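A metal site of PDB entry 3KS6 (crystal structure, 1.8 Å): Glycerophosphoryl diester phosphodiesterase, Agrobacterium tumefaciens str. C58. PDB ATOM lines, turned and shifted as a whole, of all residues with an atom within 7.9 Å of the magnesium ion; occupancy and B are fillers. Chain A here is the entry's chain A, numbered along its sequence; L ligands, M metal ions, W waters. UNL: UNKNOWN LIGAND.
Water W2 lies within hydrogen-bond range of OE1 of Glu 35 (2.5 Å), OD2 of Asp 37 (2.6 Å), NE2 of His 8 (3.1 Å) and NE of Arg 9 (3.2 Å).
The nearest printed residue that does not touch the magnesium ion is His 8 (4.2 Å).
O of Phe 36 is in hydrogen-bond range of N of Glu 105 (2.8 Å). The backbone carbonyl oxygen (O) of Glu 105 is in hydrogen-bond range of the backbone NH (N) of Leu 38 (3.4 Å). The backbone carbonyl oxygen (O) of Glu 35 lies within hydrogen-bond range of the backbone NH (N) of Arg 9, at 2.9 Å. The backbone carbonyl oxygen (O) of Asp 37 sits at hydrogen-bond distance from the backbone NH (N) of His 49 (3.2 Å).
The magnesium ion is bound by the side-chain carboxylate (OE1) of Glu 105 (2.0 Å), the side-chain carboxylate (OE2) of Glu 35 (2.1 Å), the side-chain carboxylate (OD1) of Asp 37 (2.1 Å), water W1 (2.1 Å), water W2 (2.1 Å) and an oxygen (O1) of the ligand (2.2 Å).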
ATOM      1  N   HIS A   8       8.860  26.799 -15.283  1.00  0.00           N
ATOM      2  CA  HIS A   8       9.689  25.662 -14.877  1.00  0.00           C
ATOM      3  C   HIS A   8      11.075  26.124 -14.512  1.00  0.00           C
ATOM      4  O   HIS A   8      11.814  26.602 -15.357  1.00  0.00           O
ATOM      5  CB  HIS A   8       9.714  24.606 -15.989  1.00  0.00           C
ATOM      6  CG  HIS A   8      10.351  23.303 -15.604  1.00  0.00           C
ATOM      7  ND1 HIS A   8      11.432  22.753 -16.283  1.00  0.00           N
ATOM      8  CD2 HIS A   8      10.041  22.415 -14.627  1.00  0.00           C
ATOM      9  CE1 HIS A   8      11.764  21.610 -15.710  1.00  0.00           C
ATOM     10  NE2 HIS A   8      10.916  21.358 -14.732  1.00  0.00           N
ATOM     11  N   ARG A   9      11.412  26.013 -13.236  1.00  0.00           N
ATOM     12  CA  ARG A   9      12.709  26.418 -12.735  1.00  0.00           C
ATOM     13  C   ARG A   9      12.998  27.911 -12.981  1.00  0.00           C
ATOM     14  O   ARG A   9      14.139  28.335 -13.096  1.00  0.00           O
ATOM     15  CB  ARG A   9      13.841  25.540 -13.316  1.00  0.00           C
ATOM     16  CG  ARG A   9      13.556  24.050 -13.247  1.00  0.00           C
ATOM     17  CD  ARG A   9      14.738  23.206 -13.677  1.00  0.00           C
ATOM     18  NE  ARG A   9      14.302  21.836 -13.939  1.00  0.00           N
ATOM     19  CZ  ARG A   9      14.978  20.934 -14.636  1.00  0.00           C
ATOM     20  NH1 ARG A   9      16.169  21.206 -15.164  1.00  0.00           N
ATOM     21  NH2 ARG A   9      14.435  19.734 -14.821  1.00  0.00           N
ATOM     22  N   GLU A  35       7.701  27.186 -10.671  1.00  0.00           N
ATOM     23  CA  GLU A  35       8.082  25.855 -10.224  1.00  0.00           C
ATOM     24  C   GLU A  35       9.568  25.804  -9.864  1.00  0.00           C
ATOM     25  O   GLU A  35      10.381  26.388 -10.558  1.00  0.00           O
ATOM     26  CB  GLU A  35       7.736  24.770 -11.266  1.00  0.00           C
ATOM     27  CG  GLU A  35       7.858  23.326 -10.696  1.00  0.00           C
ATOM     28  CD  GLU A  35       9.230  22.682 -10.833  1.00  0.00           C
ATOM     29  OE1 GLU A  35      10.124  23.233 -11.486  1.00  0.00           O
ATOM     30  OE2 GLU A  35       9.444  21.588 -10.244  1.00  0.00           O
ATOM     31  N   PHE A  36       9.916  25.081  -8.801  1.00  0.00           N
ATOM     32  CA  PHE A  36      11.296  24.905  -8.395  1.00  0.00           C
ATOM     33  C   PHE A  36      11.430  23.671  -7.506  1.00  0.00           C
ATOM     34  O   PHE A  36      10.435  23.189  -6.947  1.00  0.00           O
ATOM     35  CB  PHE A  36      11.785  26.163  -7.652  1.00  0.00           C
ATOM     36  CG  PHE A  36      10.960  26.473  -6.425  1.00  0.00           C
ATOM     37  CD1 PHE A  36       9.769  27.167  -6.566  1.00  0.00           C
ATOM     38  CD2 PHE A  36      11.323  25.998  -5.174  1.00  0.00           C
ATOM     39  CE1 PHE A  36       8.981  27.435  -5.492  1.00  0.00           C
ATOM     40  CE2 PHE A  36      10.549  26.256  -4.067  1.00  0.00           C
ATOM     41  CZ  PHE A  36       9.365  27.000  -4.217  1.00  0.00           C
ATOM     42  N   ASP A  37      12.662  23.199  -7.385  1.00  0.00           N
ATOM     43  CA  ASP A  37      13.014  21.991  -6.617  1.00  0.00           C
ATOM     44  C   ASP A  37      13.976  22.437  -5.512  1.00  0.00           C
ATOM     45  O   ASP A  37      14.665  23.432  -5.640  1.00  0.00           O
ATOM     46  CB  ASP A  37      13.723  20.985  -7.526  1.00  0.00           C
ATOM     47  CG  ASP A  37      13.136  20.936  -8.932  1.00  0.00           C
ATOM     48  OD1 ASP A  37      12.034  20.349  -9.118  1.00  0.00           O
ATOM     49  OD2 ASP A  37      13.768  21.490  -9.851  1.00  0.00           O
ATOM     50  N   LEU A  38      14.039  21.674  -4.430  1.00  0.00           N
ATOM     51  CA  LEU A  38      14.816  22.078  -3.252  1.00  0.00           C
ATOM     52  C   LEU A  38      15.662  20.914  -2.774  1.00  0.00           C
ATOM     53  O   LEU A  38      15.228  19.765  -2.891  1.00  0.00           O
ATOM     54  CB  LEU A  38      13.875  22.513  -2.107  1.00  0.00           C
ATOM     55  CG  LEU A  38      12.894  23.701  -2.316  1.00  0.00           C
ATOM     56  CD1 LEU A  38      11.968  23.905  -1.066  1.00  0.00           C
ATOM     57  CD2 LEU A  38      13.677  24.961  -2.634  1.00  0.00           C
ATOM     58  N   HIS A  49      17.628  24.153  -6.507  1.00  0.00           N
ATOM     59  CA  HIS A  49      18.422  23.488  -7.557  1.00  0.00           C
ATOM     60  C   HIS A  49      17.678  22.262  -8.003  1.00  0.00           C
ATOM     61  O   HIS A  49      17.043  21.597  -7.188  1.00  0.00           O
ATOM     62  CB  HIS A  49      19.785  23.093  -6.984  1.00  0.00           C
ATOM     63  CG  HIS A  49      20.861  22.956  -8.021  1.00  0.00           C
ATOM     64  ND1 HIS A  49      21.580  24.042  -8.467  1.00  0.00           N
ATOM     65  CD2 HIS A  49      21.365  21.880  -8.689  1.00  0.00           C
ATOM     66  CE1 HIS A  49      22.472  23.657  -9.361  1.00  0.00           C
ATOM     67  NE2 HIS A  49      22.361  22.343  -9.522  1.00  0.00           N
ATOM     68  N   HIS A  50      17.783  21.921  -9.290  1.00  0.00           N
ATOM     69  CA  HIS A  50      17.081  20.744  -9.771  1.00  0.00           C
ATOM     70  C   HIS A  50      17.738  19.424  -9.349  1.00  0.00           C
ATOM     71  O   HIS A  50      17.160  18.682  -8.565  1.00  0.00           O
ATOM     72  CB  HIS A  50      16.922  20.793 -11.298  1.00  0.00           C
ATOM     73  CG  HIS A  50      16.313  19.552 -11.846  1.00  0.00           C
ATOM     74  ND1 HIS A  50      16.989  18.705 -12.713  1.00  0.00           N
ATOM     75  CD2 HIS A  50      15.127  18.961 -11.585  1.00  0.00           C
ATOM     76  CE1 HIS A  50      16.225  17.654 -12.954  1.00  0.00           C
ATOM     77  NE2 HIS A  50      15.086  17.790 -12.293  1.00  0.00           N
ATOM     78  N   ARG A 103       5.055  26.468  -6.720  1.00  0.00           N
ATOM     79  CA  ARG A 103       4.879  25.041  -6.965  1.00  0.00           C
ATOM     80  C   ARG A 103       6.255  24.428  -6.576  1.00  0.00           C
ATOM     81  O   ARG A 103       7.252  24.530  -7.306  1.00  0.00           O
ATOM     82  CB  ARG A 103       4.475  24.758  -8.420  1.00  0.00           C
ATOM     83  CG  ARG A 103       4.447  23.263  -8.816  1.00  0.00           C
ATOM     84  CD  ARG A 103       4.238  23.166 -10.272  1.00  0.00           C
ATOM     85  NE  ARG A 103       4.445  21.840 -10.859  1.00  0.00           N
ATOM     86  CZ  ARG A 103       3.537  21.149 -11.534  1.00  0.00           C
ATOM     87  NH1 ARG A 103       2.305  21.616 -11.774  1.00  0.00           N
ATOM     88  NH2 ARG A 103       3.909  19.991 -12.058  1.00  0.00           N
ATOM     89  N   CYS A 104       6.298  23.843  -5.397  1.00  0.00           N
ATOM     90  CA  CYS A 104       7.524  23.362  -4.790  1.00  0.00           C
ATOM     91  C   CYS A 104       7.692  21.853  -4.974  1.00  0.00           C
ATOM     92  O   CYS A 104       6.857  21.111  -4.489  1.00  0.00           O
ATOM     93  CB  CYS A 104       7.462  23.714  -3.283  1.00  0.00           C
ATOM     94  SG  CYS A 104       8.857  23.117  -2.322  1.00  0.00           S
ATOM     95  N   GLU A 105       8.774  21.403  -5.584  1.00  0.00           N
ATOM     96  CA  GLU A 105       8.985  19.954  -5.768  1.00  0.00           C
ATOM     97  C   GLU A 105       9.972  19.416  -4.764  1.00  0.00           C
ATOM     98  O   GLU A 105      11.053  19.971  -4.591  1.00  0.00           O
ATOM     99  CB  GLU A 105       9.467  19.613  -7.193  1.00  0.00           C
ATOM    100  CG  GLU A 105       9.398  18.112  -7.472  1.00  0.00           C
ATOM    101  CD  GLU A 105       9.892  17.720  -8.850  1.00  0.00           C
ATOM    102  OE1 GLU A 105       9.905  18.584  -9.769  1.00  0.00           O
ATOM    103  OE2 GLU A 105      10.329  16.543  -8.984  1.00  0.00           O
ATOM    104  N   ILE A 106       9.580  18.332  -4.117  1.00  0.00           N
ATOM    105  CA  ILE A 106      10.394  17.585  -3.155  1.00  0.00           C
ATOM    106  C   ILE A 106      11.102  16.452  -3.903  1.00  0.00           C
ATOM    107  O   ILE A 106      10.453  15.493  -4.384  1.00  0.00           O
ATOM    108  CB  ILE A 106       9.518  16.987  -2.059  1.00  0.00           C
ATOM    109  CG1 ILE A 106       8.720  18.067  -1.343  1.00  0.00           C
ATOM    110  CG2 ILE A 106      10.380  16.209  -1.005  1.00  0.00           C
ATOM    111  CD1 ILE A 106       9.639  19.162  -0.705  1.00  0.00           C
ATOM    112  N   LYS A 107      12.418  16.595  -4.033  1.00  0.00           N
ATOM    113  CA  LYS A 107      13.310  15.674  -4.732  1.00  0.00           C
ATOM    114  C   LYS A 107      14.066  14.789  -3.742  1.00  0.00           C
ATOM    115  O   LYS A 107      14.331  15.201  -2.599  1.00  0.00           O
ATOM    116  CB  LYS A 107      14.365  16.473  -5.519  1.00  0.00           C
ATOM    117  CG  LYS A 107      13.860  17.270  -6.723  1.00  0.00           C
ATOM    118  CD  LYS A 107      13.691  16.413  -7.972  1.00  0.00           C
ATOM    119  CE  LYS A 107      14.845  16.498  -8.993  1.00  0.00           C
ATOM    120  NZ  LYS A 107      16.172  15.926  -8.590  1.00  0.00           N
ATOM    121  N   SER A 138       4.701  19.235  -4.876  1.00  0.00           N
ATOM    122  CA  SER A 138       4.685  18.178  -5.885  1.00  0.00           C
ATOM    123  C   SER A 138       5.860  17.226  -5.609  1.00  0.00           C
ATOM    124  O   SER A 138       6.806  17.619  -4.954  1.00  0.00           O
ATOM    125  CB  SER A 138       4.871  18.767  -7.274  1.00  0.00           C
ATOM    126  OG  SER A 138       6.140  19.405  -7.412  1.00  0.00           O
ATOM    127  N   PHE A 140       7.670  13.275  -7.432  1.00  0.00           N
ATOM    128  CA  PHE A 140       7.499  11.982  -8.123  1.00  0.00           C
ATOM    129  C   PHE A 140       7.382  10.826  -7.125  1.00  0.00           C
ATOM    130  O   PHE A 140       6.967   9.736  -7.519  1.00  0.00           O
ATOM    131  CB  PHE A 140       8.683  11.696  -9.033  1.00  0.00           C
ATOM    132  CG  PHE A 140       8.665  12.449 -10.325  1.00  0.00           C
ATOM    133  CD1 PHE A 140       9.225  13.722 -10.419  1.00  0.00           C
ATOM    134  CD2 PHE A 140       8.067  11.914 -11.451  1.00  0.00           C
ATOM    135  CE1 PHE A 140       9.227  14.409 -11.611  1.00  0.00           C
ATOM    136  CE2 PHE A 140       8.055  12.627 -12.653  1.00  0.00           C
ATOM    137  CZ  PHE A 140       8.648  13.855 -12.724  1.00  0.00           C
ATOM    138  N   LEU A 159       3.534  13.678  -9.343  1.00  0.00           N
ATOM    139  CA  LEU A 159       4.160  13.666 -10.655  1.00  0.00           C
ATOM    140  C   LEU A 159       4.377  12.232 -11.050  1.00  0.00           C
ATOM    141  O   LEU A 159       5.100  11.464 -10.362  1.00  0.00           O
ATOM    142  CB  LEU A 159       5.491  14.385 -10.590  1.00  0.00           C
ATOM    143  CG  LEU A 159       5.400  15.889 -10.235  1.00  0.00           C
ATOM    144  CD1 LEU A 159       6.784  16.467  -9.841  1.00  0.00           C
ATOM    145  CD2 LEU A 159       4.802  16.616 -11.425  1.00  0.00           C
ATOM    146  N   TRP A 210       3.428  18.490 -17.393  1.00  0.00           N
ATOM    147  CA  TRP A 210       4.762  19.061 -17.247  1.00  0.00           C
ATOM    148  C   TRP A 210       5.578  18.761 -18.516  1.00  0.00           C
ATOM    149  O   TRP A 210       5.153  17.985 -19.398  1.00  0.00           O
ATOM    150  CB  TRP A 210       5.477  18.609 -15.958  1.00  0.00           C
ATOM    151  CG  TRP A 210       5.409  17.143 -15.678  1.00  0.00           C
ATOM    152  CD1 TRP A 210       4.429  16.491 -15.041  1.00  0.00           C
ATOM    153  CD2 TRP A 210       6.391  16.149 -16.028  1.00  0.00           C
ATOM    154  NE1 TRP A 210       4.713  15.136 -14.978  1.00  0.00           N
ATOM    155  CE2 TRP A 210       5.931  14.914 -15.560  1.00  0.00           C
ATOM    156  CE3 TRP A 210       7.639  16.194 -16.663  1.00  0.00           C
ATOM    157  CZ2 TRP A 210       6.626  13.735 -15.752  1.00  0.00           C
ATOM    158  CZ3 TRP A 210       8.340  15.032 -16.841  1.00  0.00           C
ATOM    159  CH2 TRP A 210       7.844  13.814 -16.385  1.00  0.00           C
ATOM    160  N   THR A 230       3.736  22.988 -16.465  1.00  0.00           N
ATOM    161  CA  THR A 230       5.023  23.650 -16.306  1.00  0.00           C
ATOM    162  C   THR A 230       5.693  23.784 -17.680  1.00  0.00           C
ATOM    163  O   THR A 230       5.521  22.955 -18.574  1.00  0.00           O
ATOM    164  CB  THR A 230       5.955  22.936 -15.377  1.00  0.00           C
ATOM    165  OG1 THR A 230       6.207  21.609 -15.874  1.00  0.00           O
ATOM    166  CG2 THR A 230       5.361  22.930 -13.913  1.00  0.00           C
HETATM  167  O1  UNL L   1       9.537  19.864 -12.593  1.00  0.00           O
HETATM  168  O2  UNL L   1       8.262  18.097 -13.201  1.00  0.00           O
HETATM  169  O3  UNL L   1       7.970  20.118 -13.936  1.00  0.00           O
HETATM  170  O4  UNL L   1       6.891  19.822 -12.867  1.00  0.00           O
HETATM  171 MG    MG M   1      10.799  20.127 -10.770  1.00  0.00          MG
HETATM  172  O   HOH W   1      12.020  18.647 -11.596  1.00  0.00           O
HETATM  173  O   HOH W   2      11.972  21.575 -11.788  1.00  0.00           O
